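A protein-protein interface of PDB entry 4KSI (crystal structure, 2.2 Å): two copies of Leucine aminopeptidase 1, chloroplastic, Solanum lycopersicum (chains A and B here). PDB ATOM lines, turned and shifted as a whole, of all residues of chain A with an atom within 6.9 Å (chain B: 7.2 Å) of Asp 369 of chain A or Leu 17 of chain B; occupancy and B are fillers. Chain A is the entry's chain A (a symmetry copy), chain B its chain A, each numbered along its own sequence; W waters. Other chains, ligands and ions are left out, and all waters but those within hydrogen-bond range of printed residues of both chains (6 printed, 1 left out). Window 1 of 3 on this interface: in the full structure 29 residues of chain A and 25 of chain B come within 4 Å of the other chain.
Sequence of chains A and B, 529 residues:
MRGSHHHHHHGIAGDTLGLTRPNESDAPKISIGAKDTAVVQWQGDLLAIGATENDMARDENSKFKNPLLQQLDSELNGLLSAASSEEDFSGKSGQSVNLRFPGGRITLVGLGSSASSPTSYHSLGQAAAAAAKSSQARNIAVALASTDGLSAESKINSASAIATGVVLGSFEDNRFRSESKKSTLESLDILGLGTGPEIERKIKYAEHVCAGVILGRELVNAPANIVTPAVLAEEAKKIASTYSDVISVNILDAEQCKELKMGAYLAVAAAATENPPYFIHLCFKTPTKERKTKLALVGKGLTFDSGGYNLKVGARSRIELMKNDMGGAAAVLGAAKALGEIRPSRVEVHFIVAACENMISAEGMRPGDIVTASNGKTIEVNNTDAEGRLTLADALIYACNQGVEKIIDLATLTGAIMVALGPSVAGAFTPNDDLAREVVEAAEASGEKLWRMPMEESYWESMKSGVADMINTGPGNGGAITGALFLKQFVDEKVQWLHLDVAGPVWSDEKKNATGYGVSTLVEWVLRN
O of Gly 18 of chain B sits at hydrogen-bond distance from N of Thr 372 of chain A (2.9 Å).
The backbone carbonyl oxygen (O) of Ile 370 of chain A is in hydrogen-bond range of the side-chain hydroxyl (OG1) of Thr 20 of chain B (2.6 Å).
The side-chain hydroxyl of Thr 20 of chain B sits at hydrogen-bond distance from the side-chain hydroxyl of Thr 372 of chain A (2.8 Å).
N of Asn 225 of chain B sits at hydrogen-bond distance from OD1 of Asp 369 of chain A (3.3 Å).
ND2 of Asn 225 of chain B is in hydrogen-bond range of O of Ile 370 of chain A (2.9 Å).
OE1 of Glu 357 of chain B lies within salt-bridge range of NH1 of Arg 366 of chain A (3.0 Å).
The backbone carbonyl oxygen (O) of Asp 369 of chain A is in hydrogen-bond range of the backbone NH (N) of Val 381 of chain A, at 2.9 Å.
Leu 17 of chain B touches six residues of chain A.
Gly 368 of chain A touches just these residues of chain B: Pro 223 (3.5 Å) and Glu 320 (3.5 Å).
Of the printed residues of chain A, Asn 225 of chain B touches Arg 366, Asp 369 and Ile 370.
Of the printed residues of chain B, Gly 263 of chain A touches Gly 18 and Leu 19.
The nearest printed residue of chain B that does not touch Asp 369 of chain A is Phe 304 of chain B (5.6 Å).
Of the 19 printed residues of chain B, 12 touch a printed residue of chain A.
Hydrophobic or aromatic side chains of chain A that line the printed part of chain B: Ala 267, Ala 270, Pro 367 and Ile 370.
Among the printed residues, Asp or Glu carboxylates within 4 Å of a Lys or Arg side-chain nitrogen of the other chain: Arg 366 of chain A with Glu 357 of chain B.
No position is printed for both chains.
Of the 30 pairs that touch across the chains among the printed residues, none has its exchanged pair printed and touching as well.
Water W6 lies within hydrogen-bond range of O of Gly 368 of chain A (2.6 Å), OE2 of Glu 380 of chain A (2.7 Å) and NZ of Lys 323 of chain B (2.8 Å).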
ATOM      1  N   GLY A 263     -32.686  -8.496   9.432  1.00  0.00           N
ATOM      2  CA  GLY A 263     -31.585  -7.946   8.715  1.00  0.00           C
ATOM      3  C   GLY A 263     -30.991  -6.667   9.231  1.00  0.00           C
ATOM      4  O   GLY A 263     -29.800  -6.444   9.004  1.00  0.00           O
ATOM      5  N   LEU A 266     -28.889  -7.780  12.367  1.00  0.00           N
ATOM      6  CA  LEU A 266     -27.728  -8.623  12.006  1.00  0.00           C
ATOM      7  C   LEU A 266     -26.679  -7.809  11.225  1.00  0.00           C
ATOM      8  O   LEU A 266     -25.501  -8.117  11.252  1.00  0.00           O
ATOM      9  CB  LEU A 266     -28.185  -9.842  11.200  1.00  0.00           C
ATOM     10  CG  LEU A 266     -28.932 -10.876  12.102  1.00  0.00           C
ATOM     11  CD1 LEU A 266     -29.499 -12.020  11.249  1.00  0.00           C
ATOM     12  CD2 LEU A 266     -28.034 -11.464  13.178  1.00  0.00           C
ATOM     13  N   ALA A 267     -27.103  -6.774  10.525  1.00  0.00           N
ATOM     14  CA  ALA A 267     -26.182  -5.911   9.763  1.00  0.00           C
ATOM     15  C   ALA A 267     -25.319  -5.115  10.734  1.00  0.00           C
ATOM     16  O   ALA A 267     -24.103  -4.952  10.494  1.00  0.00           O
ATOM     17  CB  ALA A 267     -26.954  -4.950   8.844  1.00  0.00           C
ATOM     18  N   VAL A 268     -25.940  -4.586  11.816  1.00  0.00           N
ATOM     19  CA  VAL A 268     -25.166  -3.853  12.830  1.00  0.00           C
ATOM     20  C   VAL A 268     -24.125  -4.810  13.444  1.00  0.00           C
ATOM     21  O   VAL A 268     -22.928  -4.455  13.602  1.00  0.00           O
ATOM     22  CB  VAL A 268     -26.062  -3.305  13.971  1.00  0.00           C
ATOM     23  CG1 VAL A 268     -25.176  -2.706  15.071  1.00  0.00           C
ATOM     24  CG2 VAL A 268     -27.080  -2.288  13.421  1.00  0.00           C
ATOM     25  N   ALA A 270     -22.817  -7.413  12.166  1.00  0.00           N
ATOM     26  CA  ALA A 270     -21.977  -8.176  11.219  1.00  0.00           C
ATOM     27  C   ALA A 270     -20.446  -8.005  11.455  1.00  0.00           C
ATOM     28  O   ALA A 270     -19.681  -8.986  11.367  1.00  0.00           O
ATOM     29  CB  ALA A 270     -22.357  -7.824   9.746  1.00  0.00           C
ATOM     30  N   ALA A 271     -19.984  -6.793  11.768  1.00  0.00           N
ATOM     31  CA  ALA A 271     -18.528  -6.586  11.965  1.00  0.00           C
ATOM     32  C   ALA A 271     -17.917  -7.358  13.147  1.00  0.00           C
ATOM     33  O   ALA A 271     -16.757  -7.775  13.080  1.00  0.00           O
ATOM     34  CB  ALA A 271     -18.209  -5.108  12.113  1.00  0.00           C
ATOM     35  N   GLU A 363     -15.840  -7.564   7.733  1.00  0.00           N
ATOM     36  CA  GLU A 363     -17.204  -8.124   7.675  1.00  0.00           C
ATOM     37  C   GLU A 363     -18.273  -7.081   7.975  1.00  0.00           C
ATOM     38  O   GLU A 363     -19.476  -7.393   7.944  1.00  0.00           O
ATOM     39  CB  GLU A 363     -17.411  -9.336   8.655  1.00  0.00           C
ATOM     40  CG  GLU A 363     -16.631 -10.618   8.308  1.00  0.00           C
ATOM     41  CD  GLU A 363     -15.181 -10.656   8.819  1.00  0.00           C
ATOM     42  OE1 GLU A 363     -14.597  -9.608   9.241  1.00  0.00           O
ATOM     43  OE2 GLU A 363     -14.604 -11.777   8.837  1.00  0.00           O
ATOM     44  N   GLY A 364     -17.870  -5.848   8.263  1.00  0.00           N
ATOM     45  CA  GLY A 364     -18.837  -4.911   8.806  1.00  0.00           C
ATOM     46  C   GLY A 364     -19.710  -4.235   7.751  1.00  0.00           C
ATOM     47  O   GLY A 364     -19.376  -4.240   6.535  1.00  0.00           O
ATOM     48  N   MET A 365     -20.822  -3.628   8.209  1.00  0.00           N
ATOM     49  CA  MET A 365     -21.680  -2.858   7.325  1.00  0.00           C
ATOM     50  C   MET A 365     -20.996  -1.567   6.857  1.00  0.00           C
ATOM     51  O   MET A 365     -20.354  -0.894   7.648  1.00  0.00           O
ATOM     52  CB  MET A 365     -22.954  -2.514   8.093  1.00  0.00           C
ATOM     53  CG  MET A 365     -23.841  -1.494   7.419  1.00  0.00           C
ATOM     54  SD  MET A 365     -25.450  -1.495   8.251  1.00  0.00           S
ATOM     55  CE  MET A 365     -24.938  -1.100   9.911  1.00  0.00           C
ATOM     56  N   ARG A 366     -21.166  -1.194   5.590  1.00  0.00           N
ATOM     57  CA  ARG A 366     -20.556   0.020   5.105  1.00  0.00           C
ATOM     58  C   ARG A 366     -21.598   1.102   5.144  1.00  0.00           C
ATOM     59  O   ARG A 366     -22.786   0.806   4.914  1.00  0.00           O
ATOM     60  CB  ARG A 366     -20.117  -0.161   3.646  1.00  0.00           C
ATOM     61  CG  ARG A 366     -19.009  -1.200   3.348  1.00  0.00           C
ATOM     62  CD  ARG A 366     -19.236  -1.801   1.939  1.00  0.00           C
ATOM     63  NE  ARG A 366     -20.308  -2.709   2.169  1.00  0.00           N
ATOM     64  CZ  ARG A 366     -20.151  -3.978   2.513  1.00  0.00           C
ATOM     65  NH1 ARG A 366     -18.955  -4.529   2.415  1.00  0.00           N
ATOM     66  NH2 ARG A 366     -21.200  -4.660   2.942  1.00  0.00           N
ATOM     67  N   PRO A 367     -21.189   2.366   5.354  1.00  0.00           N
ATOM     68  CA  PRO A 367     -22.105   3.476   5.148  1.00  0.00           C
ATOM     69  C   PRO A 367     -22.684   3.422   3.716  1.00  0.00           C
ATOM     70  O   PRO A 367     -21.943   3.226   2.764  1.00  0.00           O
ATOM     71  CB  PRO A 367     -21.185   4.739   5.327  1.00  0.00           C
ATOM     72  CG  PRO A 367     -20.087   4.223   6.221  1.00  0.00           C
ATOM     73  CD  PRO A 367     -19.836   2.825   5.696  1.00  0.00           C
ATOM     74  N   GLY A 368     -23.995   3.622   3.554  1.00  0.00           N
ATOM     75  CA  GLY A 368     -24.614   3.556   2.221  1.00  0.00           C
ATOM     76  C   GLY A 368     -25.239   2.138   1.977  1.00  0.00           C
ATOM     77  O   GLY A 368     -26.082   2.004   1.091  1.00  0.00           O
ATOM     78  N   ASP A 369     -24.870   1.099   2.771  1.00  0.00           N
ATOM     79  CA  ASP A 369     -25.463  -0.223   2.609  1.00  0.00           C
ATOM     80  C   ASP A 369     -26.981  -0.134   2.825  1.00  0.00           C
ATOM     81  O   ASP A 369     -27.464   0.661   3.665  1.00  0.00           O
ATOM     82  CB  ASP A 369     -24.880  -1.279   3.589  1.00  0.00           C
ATOM     83  CG  ASP A 369     -23.467  -1.787   3.163  1.00  0.00           C
ATOM     84  OD1 ASP A 369     -22.932  -1.381   2.107  1.00  0.00           O
ATOM     85  OD2 ASP A 369     -22.890  -2.590   3.918  1.00  0.00           O
ATOM     86  N   ILE A 370     -27.721  -0.979   2.109  1.00  0.00           N
ATOM     87  CA  ILE A 370     -29.160  -1.060   2.335  1.00  0.00           C
ATOM     88  C   ILE A 370     -29.479  -2.329   3.078  1.00  0.00           C
ATOM     89  O   ILE A 370     -29.139  -3.413   2.585  1.00  0.00           O
ATOM     90  CB  ILE A 370     -29.958  -0.971   1.018  1.00  0.00           C
ATOM     91  CG1 ILE A 370     -29.707   0.404   0.347  1.00  0.00           C
ATOM     92  CG2 ILE A 370     -31.459  -1.254   1.294  1.00  0.00           C
ATOM     93  CD1 ILE A 370     -30.319   0.559  -1.046  1.00  0.00           C
ATOM     94  N   VAL A 371     -30.154  -2.216   4.231  1.00  0.00           N
ATOM     95  CA  VAL A 371     -30.466  -3.382   5.055  1.00  0.00           C
ATOM     96  C   VAL A 371     -31.986  -3.545   5.093  1.00  0.00           C
ATOM     97  O   VAL A 371     -32.701  -2.561   4.898  1.00  0.00           O
ATOM     98  CB  VAL A 371     -29.897  -3.250   6.485  1.00  0.00           C
ATOM     99  CG1 VAL A 371     -28.398  -2.964   6.397  1.00  0.00           C
ATOM    100  CG2 VAL A 371     -30.591  -2.125   7.255  1.00  0.00           C
ATOM    101  N   THR A 372     -32.485  -4.774   5.292  1.00  0.00           N
ATOM    102  CA  THR A 372     -33.961  -4.991   5.249  1.00  0.00           C
ATOM    103  C   THR A 372     -34.398  -5.483   6.622  1.00  0.00           C
ATOM    104  O   THR A 372     -33.909  -6.546   7.070  1.00  0.00           O
ATOM    105  CB  THR A 372     -34.278  -6.027   4.149  1.00  0.00           C
ATOM    106  OG1 THR A 372     -33.717  -5.549   2.914  1.00  0.00           O
ATOM    107  CG2 THR A 372     -35.801  -6.275   3.950  1.00  0.00           C
ATOM    108  N   ILE A 379     -33.796   0.010   4.605  1.00  0.00           N
ATOM    109  CA  ILE A 379     -33.191   1.179   5.231  1.00  0.00           C
ATOM    110  C   ILE A 379     -31.823   1.439   4.588  1.00  0.00           C
ATOM    111  O   ILE A 379     -30.963   0.491   4.522  1.00  0.00           O
ATOM    112  CB  ILE A 379     -33.008   0.953   6.746  1.00  0.00           C
ATOM    113  CG1 ILE A 379     -34.357   0.548   7.422  1.00  0.00           C
ATOM    114  CG2 ILE A 379     -32.507   2.247   7.397  1.00  0.00           C
ATOM    115  CD1 ILE A 379     -34.247  -0.544   8.474  1.00  0.00           C
ATOM    116  N   GLU A 380     -31.619   2.637   4.058  1.00  0.00           N
ATOM    117  CA  GLU A 380     -30.304   3.032   3.567  1.00  0.00           C
ATOM    118  C   GLU A 380     -29.565   3.558   4.813  1.00  0.00           C
ATOM    119  O   GLU A 380     -30.011   4.538   5.430  1.00  0.00           O
ATOM    120  CB  GLU A 380     -30.417   4.155   2.526  1.00  0.00           C
ATOM    121  CG  GLU A 380     -29.044   4.574   1.986  1.00  0.00           C
ATOM    122  CD  GLU A 380     -29.120   5.696   0.927  1.00  0.00           C
ATOM    123  OE1 GLU A 380     -30.204   6.394   0.746  1.00  0.00           O
ATOM    124  OE2 GLU A 380     -28.060   5.907   0.243  1.00  0.00           O
ATOM    125  N   VAL A 381     -28.458   2.931   5.160  1.00  0.00           N
ATOM    126  CA  VAL A 381     -27.718   3.274   6.361  1.00  0.00           C
ATOM    127  C   VAL A 381     -26.728   4.378   6.038  1.00  0.00           C
ATOM    128  O   VAL A 381     -25.557   4.080   5.799  1.00  0.00           O
ATOM    129  CB  VAL A 381     -27.021   2.030   6.998  1.00  0.00           C
ATOM    130  CG1 VAL A 381     -26.285   2.405   8.317  1.00  0.00           C
ATOM    131  CG2 VAL A 381     -28.077   0.962   7.281  1.00  0.00           C
ATOM    132  N   ASN A 382     -27.201   5.650   6.034  1.00  0.00           N
ATOM    133  CA  ASN A 382     -26.327   6.744   5.630  1.00  0.00           C
ATOM    134  C   ASN A 382     -25.374   7.092   6.745  1.00  0.00           C
ATOM    135  O   ASN A 382     -24.456   7.871   6.511  1.00  0.00           O
ATOM    136  CB  ASN A 382     -27.102   8.015   5.145  1.00  0.00           C
ATOM    137  CG  ASN A 382     -28.048   8.563   6.183  1.00  0.00           C
ATOM    138  OD1 ASN A 382     -28.724   7.799   6.895  1.00  0.00           O
ATOM    139  ND2 ASN A 382     -28.124   9.911   6.289  1.00  0.00           N
ATOM    140  N   THR A 384     -23.435   4.769   9.981  1.00  0.00           N
ATOM    141  CA  THR A 384     -23.450   3.519  10.741  1.00  0.00           C
ATOM    142  C   THR A 384     -23.414   3.743  12.228  1.00  0.00           C
ATOM    143  O   THR A 384     -23.485   2.786  12.990  1.00  0.00           O
ATOM    144  CB  THR A 384     -22.245   2.594  10.384  1.00  0.00           C
ATOM    145  OG1 THR A 384     -21.018   3.240  10.765  1.00  0.00           O
ATOM    146  CG2 THR A 384     -22.230   2.299   8.847  1.00  0.00           C
ATOM    147  N   ALA A 468     -33.741   3.536  -1.061  1.00  0.00           N
ATOM    148  CA  ALA A 468     -34.465   2.589  -0.135  1.00  0.00           C
ATOM    149  C   ALA A 468     -35.791   3.176   0.343  1.00  0.00           C
ATOM    150  O   ALA A 468     -36.135   4.282  -0.036  1.00  0.00           O
ATOM    151  CB  ALA A 468     -33.598   2.283   1.084  1.00  0.00           C
ATOM    152  N   ALA B  13     -32.445 -12.565   1.255  1.00  0.00           N
ATOM    153  CA  ALA B  13     -31.303 -13.310   0.617  1.00  0.00           C
ATOM    154  C   ALA B  13     -30.178 -13.488   1.617  1.00  0.00           C
ATOM    155  O   ALA B  13     -29.464 -12.534   1.941  1.00  0.00           O
ATOM    156  CB  ALA B  13     -30.796 -12.621  -0.652  1.00  0.00           C
ATOM    157  N   GLY B  14     -30.020 -14.737   2.062  1.00  0.00           N
ATOM    158  CA  GLY B  14     -29.225 -15.075   3.228  1.00  0.00           C
ATOM    159  C   GLY B  14     -27.720 -14.853   3.262  1.00  0.00           C
ATOM    160  O   GLY B  14     -27.159 -14.832   4.356  1.00  0.00           O
ATOM    161  N   ASP B  15     -27.051 -14.746   2.104  1.00  0.00           N
ATOM    162  CA  ASP B  15     -25.614 -14.436   2.067  1.00  0.00           C
ATOM    163  C   ASP B  15     -25.355 -12.899   1.962  1.00  0.00           C
ATOM    164  O   ASP B  15     -24.252 -12.452   2.135  1.00  0.00           O
ATOM    165  CB  ASP B  15     -24.937 -15.213   0.932  1.00  0.00           C
ATOM    166  CG  ASP B  15     -24.908 -16.750   1.181  1.00  0.00           C
ATOM    167  OD1 ASP B  15     -25.104 -17.208   2.339  1.00  0.00           O
ATOM    168  OD2 ASP B  15     -24.663 -17.510   0.215  1.00  0.00           O
ATOM    169  N   THR B  16     -26.367 -12.096   1.717  1.00  0.00           N
ATOM    170  CA  THR B  16     -26.177 -10.666   1.626  1.00  0.00           C
ATOM    171  C   THR B  16     -26.227  -9.988   3.029  1.00  0.00           C
ATOM    172  O   THR B  16     -27.129 -10.265   3.834  1.00  0.00           O
ATOM    173  CB  THR B  16     -27.225 -10.100   0.699  1.00  0.00           C
ATOM    174  OG1 THR B  16     -27.011 -10.635  -0.618  1.00  0.00           O
ATOM    175  CG2 THR B  16     -27.213  -8.577   0.675  1.00  0.00           C
ATOM    176  N   LEU B  17     -25.232  -9.142   3.335  1.00  0.00           N
ATOM    177  CA  LEU B  17     -25.279  -8.341   4.556  1.00  0.00           C
ATOM    178  C   LEU B  17     -26.654  -7.583   4.646  1.00  0.00           C
ATOM    179  O   LEU B  17     -27.053  -6.906   3.695  1.00  0.00           O
ATOM    180  CB  LEU B  17     -24.079  -7.356   4.584  1.00  0.00           C
ATOM    181  CG  LEU B  17     -24.109  -6.479   5.855  1.00  0.00           C
ATOM    182  CD1 LEU B  17     -22.682  -6.293   6.332  1.00  0.00           C
ATOM    183  CD2 LEU B  17     -24.798  -5.160   5.586  1.00  0.00           C
ATOM    184  N   GLY B  18     -27.370  -7.712   5.765  1.00  0.00           N
ATOM    185  CA  GLY B  18     -28.646  -7.027   5.905  1.00  0.00           C
ATOM    186  C   GLY B  18     -29.831  -7.731   5.197  1.00  0.00           C
ATOM    187  O   GLY B  18     -30.947  -7.241   5.291  1.00  0.00           O
ATOM    188  N   LEU B  19     -29.576  -8.898   4.562  1.00  0.00           N
ATOM    189  CA  LEU B  19     -30.621  -9.792   4.032  1.00  0.00           C
ATOM    190  C   LEU B  19     -31.399  -9.138   2.897  1.00  0.00           C
ATOM    191  O   LEU B  19     -32.478  -9.524   2.609  1.00  0.00           O
ATOM    192  CB  LEU B  19     -31.592 -10.262   5.169  1.00  0.00           C
ATOM    193  CG  LEU B  19     -30.948 -11.021   6.340  1.00  0.00           C
ATOM    194  CD1 LEU B  19     -31.963 -11.531   7.393  1.00  0.00           C
ATOM    195  CD2 LEU B  19     -30.042 -12.152   5.864  1.00  0.00           C
ATOM    196  N   THR B  20     -30.827  -8.128   2.256  1.00  0.00           N
ATOM    197  CA  THR B  20     -31.476  -7.370   1.208  1.00  0.00           C
ATOM    198  C   THR B  20     -31.499  -8.122  -0.123  1.00  0.00           C
ATOM    199  O   THR B  20     -30.476  -8.654  -0.554  1.00  0.00           O
ATOM    200  CB  THR B  20     -30.788  -5.990   1.071  1.00  0.00           C
ATOM    201  OG1 THR B  20     -30.967  -5.296   2.308  1.00  0.00           O
ATOM    202  CG2 THR B  20     -31.351  -5.149  -0.131  1.00  0.00           C
ATOM    203  N   PRO B 223     -26.179  -0.597  -3.644  1.00  0.00           N
ATOM    204  CA  PRO B 223     -25.237  -0.372  -2.560  1.00  0.00           C
ATOM    205  C   PRO B 223     -24.140  -1.429  -2.573  1.00  0.00           C
ATOM    206  O   PRO B 223     -24.287  -2.491  -3.238  1.00  0.00           O
ATOM    207  CB  PRO B 223     -26.104  -0.553  -1.318  1.00  0.00           C
ATOM    208  CG  PRO B 223     -27.209  -1.531  -1.738  1.00  0.00           C
ATOM    209  CD  PRO B 223     -27.490  -1.139  -3.189  1.00  0.00           C
ATOM    210  N   ALA B 224     -23.083  -1.177  -1.810  1.00  0.00           N
ATOM    211  CA  ALA B 224     -21.911  -2.023  -1.843  1.00  0.00           C
ATOM    212  C   ALA B 224     -22.109  -3.391  -1.179  1.00  0.00           C
ATOM    213  O   ALA B 224     -21.264  -4.269  -1.380  1.00  0.00           O
ATOM    214  CB  ALA B 224     -20.708  -1.313  -1.185  1.00  0.00           C
ATOM    215  N   ASN B 225     -23.165  -3.591  -0.388  1.00  0.00           N
ATOM    216  CA  ASN B 225     -23.452  -4.948   0.095  1.00  0.00           C
ATOM    217  C   ASN B 225     -24.113  -5.835  -0.999  1.00  0.00           C
ATOM    218  O   ASN B 225     -24.258  -7.057  -0.793  1.00  0.00           O
ATOM    219  CB  ASN B 225     -24.277  -4.968   1.405  1.00  0.00           C
ATOM    220  CG  ASN B 225     -25.599  -4.204   1.279  1.00  0.00           C
ATOM    221  OD1 ASN B 225     -25.663  -3.138   0.652  1.00  0.00           O
ATOM    222  ND2 ASN B 225     -26.660  -4.746   1.870  1.00  0.00           N
ATOM    223  N   ILE B 226     -24.507  -5.215  -2.119  1.00  0.00           N
ATOM    224  CA  ILE B 226     -25.208  -5.878  -3.230  1.00  0.00           C
ATOM    225  C   ILE B 226     -24.185  -5.953  -4.375  1.00  0.00           C
ATOM    226  O   ILE B 226     -23.866  -7.064  -4.879  1.00  0.00           O
ATOM    227  CB  ILE B 226     -26.488  -5.082  -3.651  1.00  0.00           C
ATOM    228  CG1 ILE B 226     -27.600  -5.193  -2.562  1.00  0.00           C
ATOM    229  CG2 ILE B 226     -27.028  -5.588  -5.009  1.00  0.00           C
ATOM    230  CD1 ILE B 226     -28.130  -6.616  -2.386  1.00  0.00           C
ATOM    231  N   ASN B 275     -15.042  -9.759   1.109  1.00  0.00           N
ATOM    232  CA  ASN B 275     -15.418  -9.622  -0.272  1.00  0.00           C
ATOM    233  C   ASN B 275     -14.152  -9.564  -1.123  1.00  0.00           C
ATOM    234  O   ASN B 275     -13.651  -8.463  -1.365  1.00  0.00           O
ATOM    235  CB  ASN B 275     -16.283  -8.345  -0.440  1.00  0.00           C
ATOM    236  CG  ASN B 275     -17.623  -8.474   0.295  1.00  0.00           C
ATOM    237  OD1 ASN B 275     -17.931  -7.679   1.197  1.00  0.00           O
ATOM    238  ND2 ASN B 275     -18.378  -9.525  -0.016  1.00  0.00           N
ATOM    239  N   THR B 303     -15.672  -0.899  -5.287  1.00  0.00           N
ATOM    240  CA  THR B 303     -17.073  -1.094  -5.055  1.00  0.00           C
ATOM    241  C   THR B 303     -17.525  -0.427  -3.746  1.00  0.00           C
ATOM    242  O   THR B 303     -18.748  -0.150  -3.537  1.00  0.00           O
ATOM    243  CB  THR B 303     -17.431  -2.600  -5.085  1.00  0.00           C
ATOM    244  OG1 THR B 303     -16.756  -3.267  -4.018  1.00  0.00           O
ATOM    245  CG2 THR B 303     -17.091  -3.263  -6.457  1.00  0.00           C
ATOM    246  N   PHE B 304     -16.562  -0.208  -2.857  1.00  0.00           N
ATOM    247  CA  PHE B 304     -16.725   0.706  -1.722  1.00  0.00           C
ATOM    248  C   PHE B 304     -15.368   1.240  -1.308  1.00  0.00           C
ATOM    249  O   PHE B 304     -14.354   0.525  -1.373  1.00  0.00           O
ATOM    250  CB  PHE B 304     -17.397   0.074  -0.482  1.00  0.00           C
ATOM    251  CG  PHE B 304     -17.739   1.110   0.559  1.00  0.00           C
ATOM    252  CD1 PHE B 304     -18.787   2.022   0.330  1.00  0.00           C
ATOM    253  CD2 PHE B 304     -16.934   1.285   1.686  1.00  0.00           C
ATOM    254  CE1 PHE B 304     -19.054   3.063   1.247  1.00  0.00           C
ATOM    255  CE2 PHE B 304     -17.211   2.270   2.614  1.00  0.00           C
ATOM    256  CZ  PHE B 304     -18.269   3.167   2.385  1.00  0.00           C
ATOM    257  N   GLU B 320     -20.783   7.888   2.983  1.00  0.00           N
ATOM    258  CA  GLU B 320     -22.020   7.206   2.734  1.00  0.00           C
ATOM    259  C   GLU B 320     -22.368   7.139   1.221  1.00  0.00           C
ATOM    260  O   GLU B 320     -23.313   6.465   0.889  1.00  0.00           O
ATOM    261  CB  GLU B 320     -23.157   7.849   3.554  1.00  0.00           C
ATOM    262  CG  GLU B 320     -23.616   9.253   3.065  1.00  0.00           C
ATOM    263  CD  GLU B 320     -22.607  10.419   3.340  1.00  0.00           C
ATOM    264  OE1 GLU B 320     -21.612  10.320   4.160  1.00  0.00           O
ATOM    265  OE2 GLU B 320     -22.799  11.489   2.727  1.00  0.00           O
ATOM    266  N   LYS B 323     -20.213   3.871  -2.434  1.00  0.00           N
ATOM    267  CA  LYS B 323     -20.586   2.843  -3.422  1.00  0.00           C
ATOM    268  C   LYS B 323     -20.335   3.398  -4.846  1.00  0.00           C
ATOM    269  O   LYS B 323     -20.288   2.608  -5.805  1.00  0.00           O
ATOM    270  CB  LYS B 323     -22.084   2.479  -3.303  1.00  0.00           C
ATOM    271  CG  LYS B 323     -23.030   3.647  -3.669  1.00  0.00           C
ATOM    272  CD  LYS B 323     -24.523   3.268  -3.481  1.00  0.00           C
ATOM    273  CE  LYS B 323     -25.429   4.452  -3.892  1.00  0.00           C
ATOM    274  NZ  LYS B 323     -26.876   4.122  -3.542  1.00  0.00           N
ATOM    275  N   GLU B 357     -12.794  -3.712  -2.707  1.00  0.00           N
ATOM    276  CA  GLU B 357     -13.303  -2.685  -1.787  1.00  0.00           C
ATOM    277  C   GLU B 357     -12.195  -2.293  -0.824  1.00  0.00           C
ATOM    278  O   GLU B 357     -11.315  -3.096  -0.592  1.00  0.00           O
ATOM    279  CB  GLU B 357     -14.621  -3.097  -1.069  1.00  0.00           C
ATOM    280  CG  GLU B 357     -14.556  -4.377  -0.313  1.00  0.00           C
ATOM    281  CD  GLU B 357     -15.821  -4.664   0.493  1.00  0.00           C
ATOM    282  OE1 GLU B 357     -16.876  -3.993   0.287  1.00  0.00           O
ATOM    283  OE2 GLU B 357     -15.770  -5.604   1.329  1.00  0.00           O
ATOM    284  N   MET B 359     -11.265  -1.459   2.717  1.00  0.00           N
ATOM    285  CA  MET B 359     -11.828  -1.651   4.066  1.00  0.00           C
ATOM    286  C   MET B 359     -10.801  -1.471   5.201  1.00  0.00           C
ATOM    287  O   MET B 359      -9.648  -1.105   4.974  1.00  0.00           O
ATOM    288  CB  MET B 359     -12.463  -3.054   4.122  1.00  0.00           C
ATOM    289  CG  MET B 359     -13.556  -3.215   3.067  1.00  0.00           C
ATOM    290  SD  MET B 359     -15.044  -2.196   3.418  1.00  0.00           S
ATOM    291  CE  MET B 359     -15.946  -3.397   4.432  1.00  0.00           C
HETATM  292  O   HOH W   1     -21.997   9.241   6.794  1.00  0.00           O
HETATM  293  O   HOH W   2     -22.977   0.967   0.232  1.00  0.00           O
HETATM  294  O   HOH W   3     -26.086   6.914   1.779  1.00  0.00           O
HETATM  295  O   HOH W   4     -22.203   4.052  -0.321  1.00  0.00           O
HETATM  296  O   HOH W   5     -27.819   6.866  -2.173  1.00  0.00           O
HETATM  297  O   HOH W   6     -26.926   3.677  -0.752  1.00  0.00           O
